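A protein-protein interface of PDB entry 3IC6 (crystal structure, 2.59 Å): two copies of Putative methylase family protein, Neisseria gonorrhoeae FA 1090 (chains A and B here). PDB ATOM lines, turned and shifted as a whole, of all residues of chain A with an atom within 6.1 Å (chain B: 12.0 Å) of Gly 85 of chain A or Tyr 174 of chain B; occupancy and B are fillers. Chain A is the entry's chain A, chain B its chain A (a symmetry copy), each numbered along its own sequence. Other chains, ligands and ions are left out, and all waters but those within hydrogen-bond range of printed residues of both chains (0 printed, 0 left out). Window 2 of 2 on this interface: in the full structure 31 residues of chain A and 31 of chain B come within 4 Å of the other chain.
The backbone NH (N) of Ser 176 of chain B lies within hydrogen-bond range of the side-chain hydroxyl (OG1) of Thr 40 of chain A (3.0 Å).
O of Thr 40 of chain A sits at hydrogen-bond distance from N of Asn 171 of chain B.
The backbone carbonyl oxygen of Lys 39 of chain A lies within hydrogen-bond range of the side-chain amide nitrogen of Asn 171 of chain B (2.9 Å).
The side-chain sulfur of Met 41 of chain A lies close to the backbone carbonyl oxygen of Asn 169 of chain B (3.5 Å).
The side-chain hydroxyl of Ser 176 of chain B sits at hydrogen-bond distance from the guanidinium group of Arg 36 of chain A (2.9 Å).
Of chain B, only Tyr 174 comes within 4 Å of Gly 85 of chain A.
Of chain A, only Arg 36 (3.6 Å), Lys 39 (3.6 Å), Thr 40 (3.5 Å), Ala 83 (3.8 Å), Ser 84 (3.8 Å), Gly 85 (3.5 Å) and Ala 86 (3.7 Å) come within 4 Å of Tyr 174 of chain B.
Of chain B, only Asn 171 (2.9 Å) and Tyr 174 (3.6 Å) come within 4 Å of Lys 39 of chain A.
Ser 84 of chain A touches just one residue of chain B: Tyr 174 (3.8 Å).
Ala 86 of chain A touches one residue of chain B.
No residue of chain B comes within 4 Å of Ala 87 of chain A.
No residue of chain B comes within 4 Å of Asp 88 of chain A.
Printed residues of chain A within 4 Å of Asn 171 of chain B: Lys 39 (2.9 Å), Thr 40 (2.8 Å) and Gly 42 (3.7 Å).
Of the printed residues of chain A, Ile 168 of chain B touches Met 41 (3.9 Å).
Of the printed residues of chain A, Asn 169 of chain B touches Met 41.
The side-chain amino group (NZ) of Lys 39 of chain A is in salt-bridge range of the side-chain carboxylate (OD1) of Asp 88 of chain A (3.1 Å).
The backbone NH (N) of Gln 181 of chain B is in hydrogen-bond range of the side-chain amide oxygen (OD1) of Asn 178 of chain B (2.8 Å).
The side-chain amide oxygen of Asn 171 of chain B is in hydrogen-bond range of the backbone NH of Asp 173 of chain B (2.9 Å).
NZ of Lys 39 of chain A lies within hydrogen-bond range of O of Gly 85 of chain A (2.7 Å).
The backbone carbonyl oxygen (O) of Arg 36 of chain A lies within hydrogen-bond range of the side-chain hydroxyl (OG1) of Thr 40 of chain A (2.8 Å).
NH2 of Arg 36 of chain A touches N of Asn 178 of chain B (3.6 Å).
CG of Tyr 174 of chain B touches CD of Lys 39 of chain A, 3.6 Å away.
Thr 40 of chain A touches Gly 170 of chain B.
Thr 40 of chain A touches Tyr 174 of chain B.
CD1 of Phe 175 of chain B touches CG2 of Thr 40 of chain A, 3.5 Å away.
Met 41 of chain A touches Ile 168 of chain B.
Gly 42 of chain A touches Asn 171 of chain B (N to CB, 3.7 Å).
OH of Tyr 174 of chain B touches O of Ala 83 of chain A, at 3.8 Å.
Gly 85 of chain A touches Tyr 174 of chain B.
OH of Tyr 174 of chain B touches N of Ala 86 of chain A, 3.7 Å away.
Of the 14 printed residues of chain B, 9 touch a printed residue of chain A.
Hydrophobic or aromatic side chains of chain B within 4 Å of the printed part of chain A: Ile 168, Tyr 174 and Phe 175.
Printed residues of chain A that touch a printed residue of chain B: Arg 36, Lys 39, Thr 40, Met 41, Gly 42, Ala 83, Ser 84, Gly 85 and Ala 86.
Along chain A the printed residues that touch a printed residue of chain B span positions 36 to 86.
Among the printed residues, 18 pairs touch across the chains.
Among the printed residues, no Asp or Glu carboxylate lies within 4 Å of a Lys or Arg side-chain nitrogen of the other chain.
No position is printed for both chains.
Of the 18 pairs that touch across the chains among the printed residues, none has its exchanged pair printed and touching as well.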
ATOM      1  N   ALA A  35     -14.984  29.425 -26.657  1.00  0.00           N
ATOM      2  CA  ALA A  35     -15.986  28.521 -27.228  1.00  0.00           C
ATOM      3  C   ALA A  35     -15.937  27.126 -26.583  1.00  0.00           C
ATOM      4  O   ALA A  35     -16.971  26.572 -26.192  1.00  0.00           O
ATOM      5  CB  ALA A  35     -15.823  28.424 -28.758  1.00  0.00           C
ATOM      6  N   ARG A  36     -14.731  26.574 -26.461  1.00  0.00           N
ATOM      7  CA  ARG A  36     -14.522  25.226 -25.881  1.00  0.00           C
ATOM      8  C   ARG A  36     -15.007  25.176 -24.410  1.00  0.00           C
ATOM      9  O   ARG A  36     -15.801  24.306 -24.031  1.00  0.00           O
ATOM     10  CB  ARG A  36     -13.047  24.837 -26.018  1.00  0.00           C
ATOM     11  CG  ARG A  36     -12.767  23.367 -26.068  1.00  0.00           C
ATOM     12  CD  ARG A  36     -11.272  23.094 -25.901  1.00  0.00           C
ATOM     13  NE  ARG A  36     -11.079  21.899 -25.099  1.00  0.00           N
ATOM     14  CZ  ARG A  36      -9.900  21.442 -24.661  1.00  0.00           C
ATOM     15  NH1 ARG A  36      -8.781  22.106 -24.956  1.00  0.00           N
ATOM     16  NH2 ARG A  36      -9.842  20.306 -23.937  1.00  0.00           N
ATOM     17  N   LYS A  39     -19.086  25.582 -24.392  1.00  0.00           N
ATOM     18  CA  LYS A  39     -19.928  24.473 -24.832  1.00  0.00           C
ATOM     19  C   LYS A  39     -19.929  23.332 -23.807  1.00  0.00           C
ATOM     20  O   LYS A  39     -20.974  22.729 -23.528  1.00  0.00           O
ATOM     21  CB  LYS A  39     -19.488  23.975 -26.202  1.00  0.00           C
ATOM     22  CG  LYS A  39     -20.583  23.285 -26.960  1.00  0.00           C
ATOM     23  CD  LYS A  39     -20.015  22.516 -28.116  1.00  0.00           C
ATOM     24  CE  LYS A  39     -21.113  22.123 -29.067  1.00  0.00           C
ATOM     25  NZ  LYS A  39     -20.575  21.416 -30.266  1.00  0.00           N
ATOM     26  N   THR A  40     -18.749  23.070 -23.250  1.00  0.00           N
ATOM     27  CA  THR A  40     -18.550  22.115 -22.184  1.00  0.00           C
ATOM     28  C   THR A  40     -19.467  22.389 -20.997  1.00  0.00           C
ATOM     29  O   THR A  40     -19.798  21.480 -20.231  1.00  0.00           O
ATOM     30  CB  THR A  40     -17.093  22.192 -21.722  1.00  0.00           C
ATOM     31  OG1 THR A  40     -16.264  21.805 -22.810  1.00  0.00           O
ATOM     32  CG2 THR A  40     -16.815  21.286 -20.560  1.00  0.00           C
ATOM     33  N   MET A  41     -19.853  23.648 -20.818  1.00  0.00           N
ATOM     34  CA  MET A  41     -20.655  24.012 -19.660  1.00  0.00           C
ATOM     35  C   MET A  41     -22.041  24.360 -20.142  1.00  0.00           C
ATOM     36  O   MET A  41     -22.820  24.954 -19.412  1.00  0.00           O
ATOM     37  CB  MET A  41     -20.017  25.145 -18.859  1.00  0.00           C
ATOM     38  CG  MET A  41     -18.766  24.730 -18.119  1.00  0.00           C
ATOM     39  SD  MET A  41     -19.119  23.232 -16.938  1.00  0.00           S
ATOM     40  CE  MET A  41     -17.316  22.781 -16.371  1.00  0.00           C
ATOM     41  N   GLY A  42     -22.341  23.961 -21.373  1.00  0.00           N
ATOM     42  CA  GLY A  42     -23.672  24.118 -21.935  1.00  0.00           C
ATOM     43  C   GLY A  42     -24.107  25.511 -22.362  1.00  0.00           C
ATOM     44  O   GLY A  42     -25.302  25.788 -22.452  1.00  0.00           O
ATOM     45  N   ALA A  83     -11.068  25.812 -31.014  1.00  0.00           N
ATOM     46  CA  ALA A  83     -12.424  25.551 -30.575  1.00  0.00           C
ATOM     47  C   ALA A  83     -12.740  24.056 -30.509  1.00  0.00           C
ATOM     48  O   ALA A  83     -13.629  23.664 -29.743  1.00  0.00           O
ATOM     49  CB  ALA A  83     -13.419  26.264 -31.451  1.00  0.00           C
ATOM     50  N   SER A  84     -12.015  23.236 -31.290  1.00  0.00           N
ATOM     51  CA  SER A  84     -12.297  21.782 -31.445  1.00  0.00           C
ATOM     52  C   SER A  84     -13.709  21.492 -31.957  1.00  0.00           C
ATOM     53  O   SER A  84     -14.136  22.029 -32.983  1.00  0.00           O
ATOM     54  CB  SER A  84     -12.095  21.028 -30.119  1.00  0.00           C
ATOM     55  OG  SER A  84     -10.753  20.634 -29.954  1.00  0.00           O
ATOM     56  N   GLY A  85     -14.432  20.654 -31.210  1.00  0.00           N
ATOM     57  CA  GLY A  85     -15.824  20.344 -31.498  1.00  0.00           C
ATOM     58  C   GLY A  85     -16.789  21.422 -31.037  1.00  0.00           C
ATOM     59  O   GLY A  85     -18.002  21.237 -31.106  1.00  0.00           O
ATOM     60  N   ALA A  86     -16.253  22.544 -30.562  1.00  0.00           N
ATOM     61  CA  ALA A  86     -17.072  23.718 -30.279  1.00  0.00           C
ATOM     62  C   ALA A  86     -17.003  24.756 -31.401  1.00  0.00           C
ATOM     63  O   ALA A  86     -17.375  25.898 -31.200  1.00  0.00           O
ATOM     64  CB  ALA A  86     -16.682  24.342 -28.940  1.00  0.00           C
ATOM     65  N   ALA A  87     -16.538  24.355 -32.585  1.00  0.00           N
ATOM     66  CA  ALA A  87     -16.399  25.300 -33.708  1.00  0.00           C
ATOM     67  C   ALA A  87     -17.749  25.919 -34.101  1.00  0.00           C
ATOM     68  O   ALA A  87     -17.823  27.108 -34.433  1.00  0.00           O
ATOM     69  CB  ALA A  87     -15.699  24.660 -34.900  1.00  0.00           C
ATOM     70  N   ASP A  88     -18.817  25.132 -34.022  1.00  0.00           N
ATOM     71  CA  ASP A  88     -20.170  25.656 -34.235  1.00  0.00           C
ATOM     72  C   ASP A  88     -20.425  26.951 -33.457  1.00  0.00           C
ATOM     73  O   ASP A  88     -20.896  27.933 -34.036  1.00  0.00           O
ATOM     74  CB  ASP A  88     -21.255  24.600 -33.940  1.00  0.00           C
ATOM     75  CG  ASP A  88     -21.167  24.024 -32.527  1.00  0.00           C
ATOM     76  OD1 ASP A  88     -20.057  23.920 -31.965  1.00  0.00           O
ATOM     77  OD2 ASP A  88     -22.220  23.649 -31.975  1.00  0.00           O
ATOM     78  N   SER B 114     -14.352  10.494 -14.610  1.00  0.00           N
ATOM     79  CA  SER B 114     -15.660  10.642 -15.274  1.00  0.00           C
ATOM     80  C   SER B 114     -16.462   9.348 -15.101  1.00  0.00           C
ATOM     81  O   SER B 114     -15.907   8.344 -14.625  1.00  0.00           O
ATOM     82  CB  SER B 114     -15.481  10.958 -16.763  1.00  0.00           C
ATOM     83  OG  SER B 114     -14.695   9.969 -17.403  1.00  0.00           O
ATOM     84  N   THR B 167     -16.341  14.212  -9.620  1.00  0.00           N
ATOM     85  CA  THR B 167     -16.543  14.529 -11.009  1.00  0.00           C
ATOM     86  C   THR B 167     -16.882  16.009 -11.240  1.00  0.00           C
ATOM     87  O   THR B 167     -17.408  16.687 -10.355  1.00  0.00           O
ATOM     88  CB  THR B 167     -17.582  13.620 -11.625  1.00  0.00           C
ATOM     89  OG1 THR B 167     -17.398  13.632 -13.043  1.00  0.00           O
ATOM     90  CG2 THR B 167     -18.977  14.073 -11.278  1.00  0.00           C
ATOM     91  N   ILE B 168     -16.548  16.502 -12.432  1.00  0.00           N
ATOM     92  CA  ILE B 168     -16.923  17.834 -12.841  1.00  0.00           C
ATOM     93  C   ILE B 168     -18.012  17.688 -13.887  1.00  0.00           C
ATOM     94  O   ILE B 168     -17.765  17.154 -14.965  1.00  0.00           O
ATOM     95  CB  ILE B 168     -15.706  18.603 -13.412  1.00  0.00           C
ATOM     96  CG1 ILE B 168     -14.654  18.801 -12.310  1.00  0.00           C
ATOM     97  CG2 ILE B 168     -16.131  19.953 -14.015  1.00  0.00           C
ATOM     98  CD1 ILE B 168     -13.324  19.356 -12.789  1.00  0.00           C
ATOM     99  N   ASN B 169     -19.223  18.145 -13.578  1.00  0.00           N
ATOM    100  CA  ASN B 169     -20.328  18.025 -14.540  1.00  0.00           C
ATOM    101  C   ASN B 169     -20.315  19.113 -15.581  1.00  0.00           C
ATOM    102  O   ASN B 169     -19.732  20.185 -15.380  1.00  0.00           O
ATOM    103  CB  ASN B 169     -21.684  18.055 -13.834  1.00  0.00           C
ATOM    104  CG  ASN B 169     -21.851  16.921 -12.823  1.00  0.00           C
ATOM    105  OD1 ASN B 169     -22.332  17.164 -11.708  1.00  0.00           O
ATOM    106  ND2 ASN B 169     -21.446  15.678 -13.200  1.00  0.00           N
ATOM    107  N   GLY B 170     -20.990  18.845 -16.682  1.00  0.00           N
ATOM    108  CA  GLY B 170     -21.140  19.817 -17.721  1.00  0.00           C
ATOM    109  C   GLY B 170     -22.160  19.352 -18.726  1.00  0.00           C
ATOM    110  O   GLY B 170     -23.094  18.615 -18.404  1.00  0.00           O
ATOM    111  N   ASN B 171     -21.989  19.804 -19.951  1.00  0.00           N
ATOM    112  CA  ASN B 171     -22.898  19.500 -21.022  1.00  0.00           C
ATOM    113  C   ASN B 171     -22.808  17.987 -21.344  1.00  0.00           C
ATOM    114  O   ASN B 171     -21.719  17.462 -21.663  1.00  0.00           O
ATOM    115  CB  ASN B 171     -22.533  20.397 -22.199  1.00  0.00           C
ATOM    116  CG  ASN B 171     -23.324  20.114 -23.446  1.00  0.00           C
ATOM    117  OD1 ASN B 171     -24.284  19.333 -23.458  1.00  0.00           O
ATOM    118  ND2 ASN B 171     -22.919  20.763 -24.531  1.00  0.00           N
ATOM    119  N   PRO B 172     -23.949  17.273 -21.225  1.00  0.00           N
ATOM    120  CA  PRO B 172     -23.980  15.851 -21.529  1.00  0.00           C
ATOM    121  C   PRO B 172     -23.611  15.541 -22.979  1.00  0.00           C
ATOM    122  O   PRO B 172     -23.080  14.466 -23.227  1.00  0.00           O
ATOM    123  CB  PRO B 172     -25.428  15.459 -21.228  1.00  0.00           C
ATOM    124  CG  PRO B 172     -26.200  16.747 -21.315  1.00  0.00           C
ATOM    125  CD  PRO B 172     -25.261  17.752 -20.745  1.00  0.00           C
ATOM    126  N   ASP B 173     -23.847  16.468 -23.919  1.00  0.00           N
ATOM    127  CA  ASP B 173     -23.599  16.211 -25.370  1.00  0.00           C
ATOM    128  C   ASP B 173     -22.198  16.573 -25.863  1.00  0.00           C
ATOM    129  O   ASP B 173     -21.821  16.248 -26.992  1.00  0.00           O
ATOM    130  CB  ASP B 173     -24.588  16.985 -26.237  1.00  0.00           C
ATOM    131  CG  ASP B 173     -26.039  16.642 -25.945  1.00  0.00           C
ATOM    132  OD1 ASP B 173     -26.327  15.653 -25.244  1.00  0.00           O
ATOM    133  OD2 ASP B 173     -26.918  17.375 -26.435  1.00  0.00           O
ATOM    134  N   TYR B 174     -21.453  17.286 -25.027  1.00  0.00           N
ATOM    135  CA  TYR B 174     -20.108  17.745 -25.366  1.00  0.00           C
ATOM    136  C   TYR B 174     -19.417  18.184 -24.104  1.00  0.00           C
ATOM    137  O   TYR B 174     -19.929  19.026 -23.377  1.00  0.00           O
ATOM    138  CB  TYR B 174     -20.143  18.926 -26.335  1.00  0.00           C
ATOM    139  CG  TYR B 174     -18.768  19.461 -26.644  1.00  0.00           C
ATOM    140  CD1 TYR B 174     -18.080  19.030 -27.773  1.00  0.00           C
ATOM    141  CD2 TYR B 174     -18.141  20.399 -25.803  1.00  0.00           C
ATOM    142  CE1 TYR B 174     -16.804  19.513 -28.070  1.00  0.00           C
ATOM    143  CE2 TYR B 174     -16.867  20.879 -26.086  1.00  0.00           C
ATOM    144  CZ  TYR B 174     -16.204  20.432 -27.224  1.00  0.00           C
ATOM    145  OH  TYR B 174     -14.939  20.897 -27.536  1.00  0.00           O
ATOM    146  N   PHE B 175     -18.250  17.624 -23.842  1.00  0.00           N
ATOM    147  CA  PHE B 175     -17.541  17.954 -22.642  1.00  0.00           C
ATOM    148  C   PHE B 175     -16.071  17.888 -22.966  1.00  0.00           C
ATOM    149  O   PHE B 175     -15.595  16.850 -23.352  1.00  0.00           O
ATOM    150  CB  PHE B 175     -17.877  16.966 -21.542  1.00  0.00           C
ATOM    151  CG  PHE B 175     -17.302  17.335 -20.213  1.00  0.00           C
ATOM    152  CD1 PHE B 175     -18.003  18.178 -19.345  1.00  0.00           C
ATOM    153  CD2 PHE B 175     -16.059  16.852 -19.821  1.00  0.00           C
ATOM    154  CE1 PHE B 175     -17.468  18.537 -18.109  1.00  0.00           C
ATOM    155  CE2 PHE B 175     -15.513  17.178 -18.577  1.00  0.00           C
ATOM    156  CZ  PHE B 175     -16.207  18.035 -17.720  1.00  0.00           C
ATOM    157  N   SER B 176     -15.341  18.983 -22.819  1.00  0.00           N
ATOM    158  CA  SER B 176     -13.946  18.958 -23.188  1.00  0.00           C
ATOM    159  C   SER B 176     -13.146  19.851 -22.278  1.00  0.00           C
ATOM    160  O   SER B 176     -13.025  21.029 -22.529  1.00  0.00           O
ATOM    161  CB  SER B 176     -13.779  19.381 -24.648  1.00  0.00           C
ATOM    162  OG  SER B 176     -12.423  19.296 -25.025  1.00  0.00           O
ATOM    163  N   LEU B 177     -12.592  19.279 -21.227  1.00  0.00           N
ATOM    164  CA  LEU B 177     -11.950  20.057 -20.200  1.00  0.00           C
ATOM    165  C   LEU B 177     -10.555  19.512 -20.021  1.00  0.00           C
ATOM    166  O   LEU B 177     -10.394  18.381 -19.568  1.00  0.00           O
ATOM    167  CB  LEU B 177     -12.727  19.899 -18.883  1.00  0.00           C
ATOM    168  CG  LEU B 177     -12.426  20.910 -17.769  1.00  0.00           C
ATOM    169  CD1 LEU B 177     -13.295  22.085 -17.999  1.00  0.00           C
ATOM    170  CD2 LEU B 177     -12.729  20.337 -16.397  1.00  0.00           C
ATOM    171  N   ASN B 178      -9.531  20.271 -20.359  1.00  0.00           N
ATOM    172  CA  ASN B 178      -8.205  19.699 -20.211  1.00  0.00           C
ATOM    173  C   ASN B 178      -7.731  19.636 -18.753  1.00  0.00           C
ATOM    174  O   ASN B 178      -8.428  20.082 -17.833  1.00  0.00           O
ATOM    175  CB  ASN B 178      -7.184  20.356 -21.164  1.00  0.00           C
ATOM    176  CG  ASN B 178      -6.852  21.803 -20.801  1.00  0.00           C
ATOM    177  OD1 ASN B 178      -6.797  22.193 -19.623  1.00  0.00           O
ATOM    178  ND2 ASN B 178      -6.599  22.593 -21.823  1.00  0.00           N
ATOM    179  N   GLN B 181      -7.340  23.034 -17.039  1.00  0.00           N
ATOM    180  CA  GLN B 181      -8.621  23.653 -16.751  1.00  0.00           C
ATOM    181  C   GLN B 181      -9.277  22.938 -15.559  1.00  0.00           C
ATOM    182  O   GLN B 181      -9.899  23.587 -14.700  1.00  0.00           O
ATOM    183  CB  GLN B 181      -9.541  23.659 -17.976  1.00  0.00           C
ATOM    184  CG  GLN B 181      -9.053  24.473 -19.179  1.00  0.00           C
ATOM    185  CD  GLN B 181      -9.901  24.194 -20.471  1.00  0.00           C
ATOM    186  OE1 GLN B 181     -10.019  23.036 -20.953  1.00  0.00           O
ATOM    187  NE2 GLN B 181     -10.495  25.278 -21.038  1.00  0.00           N
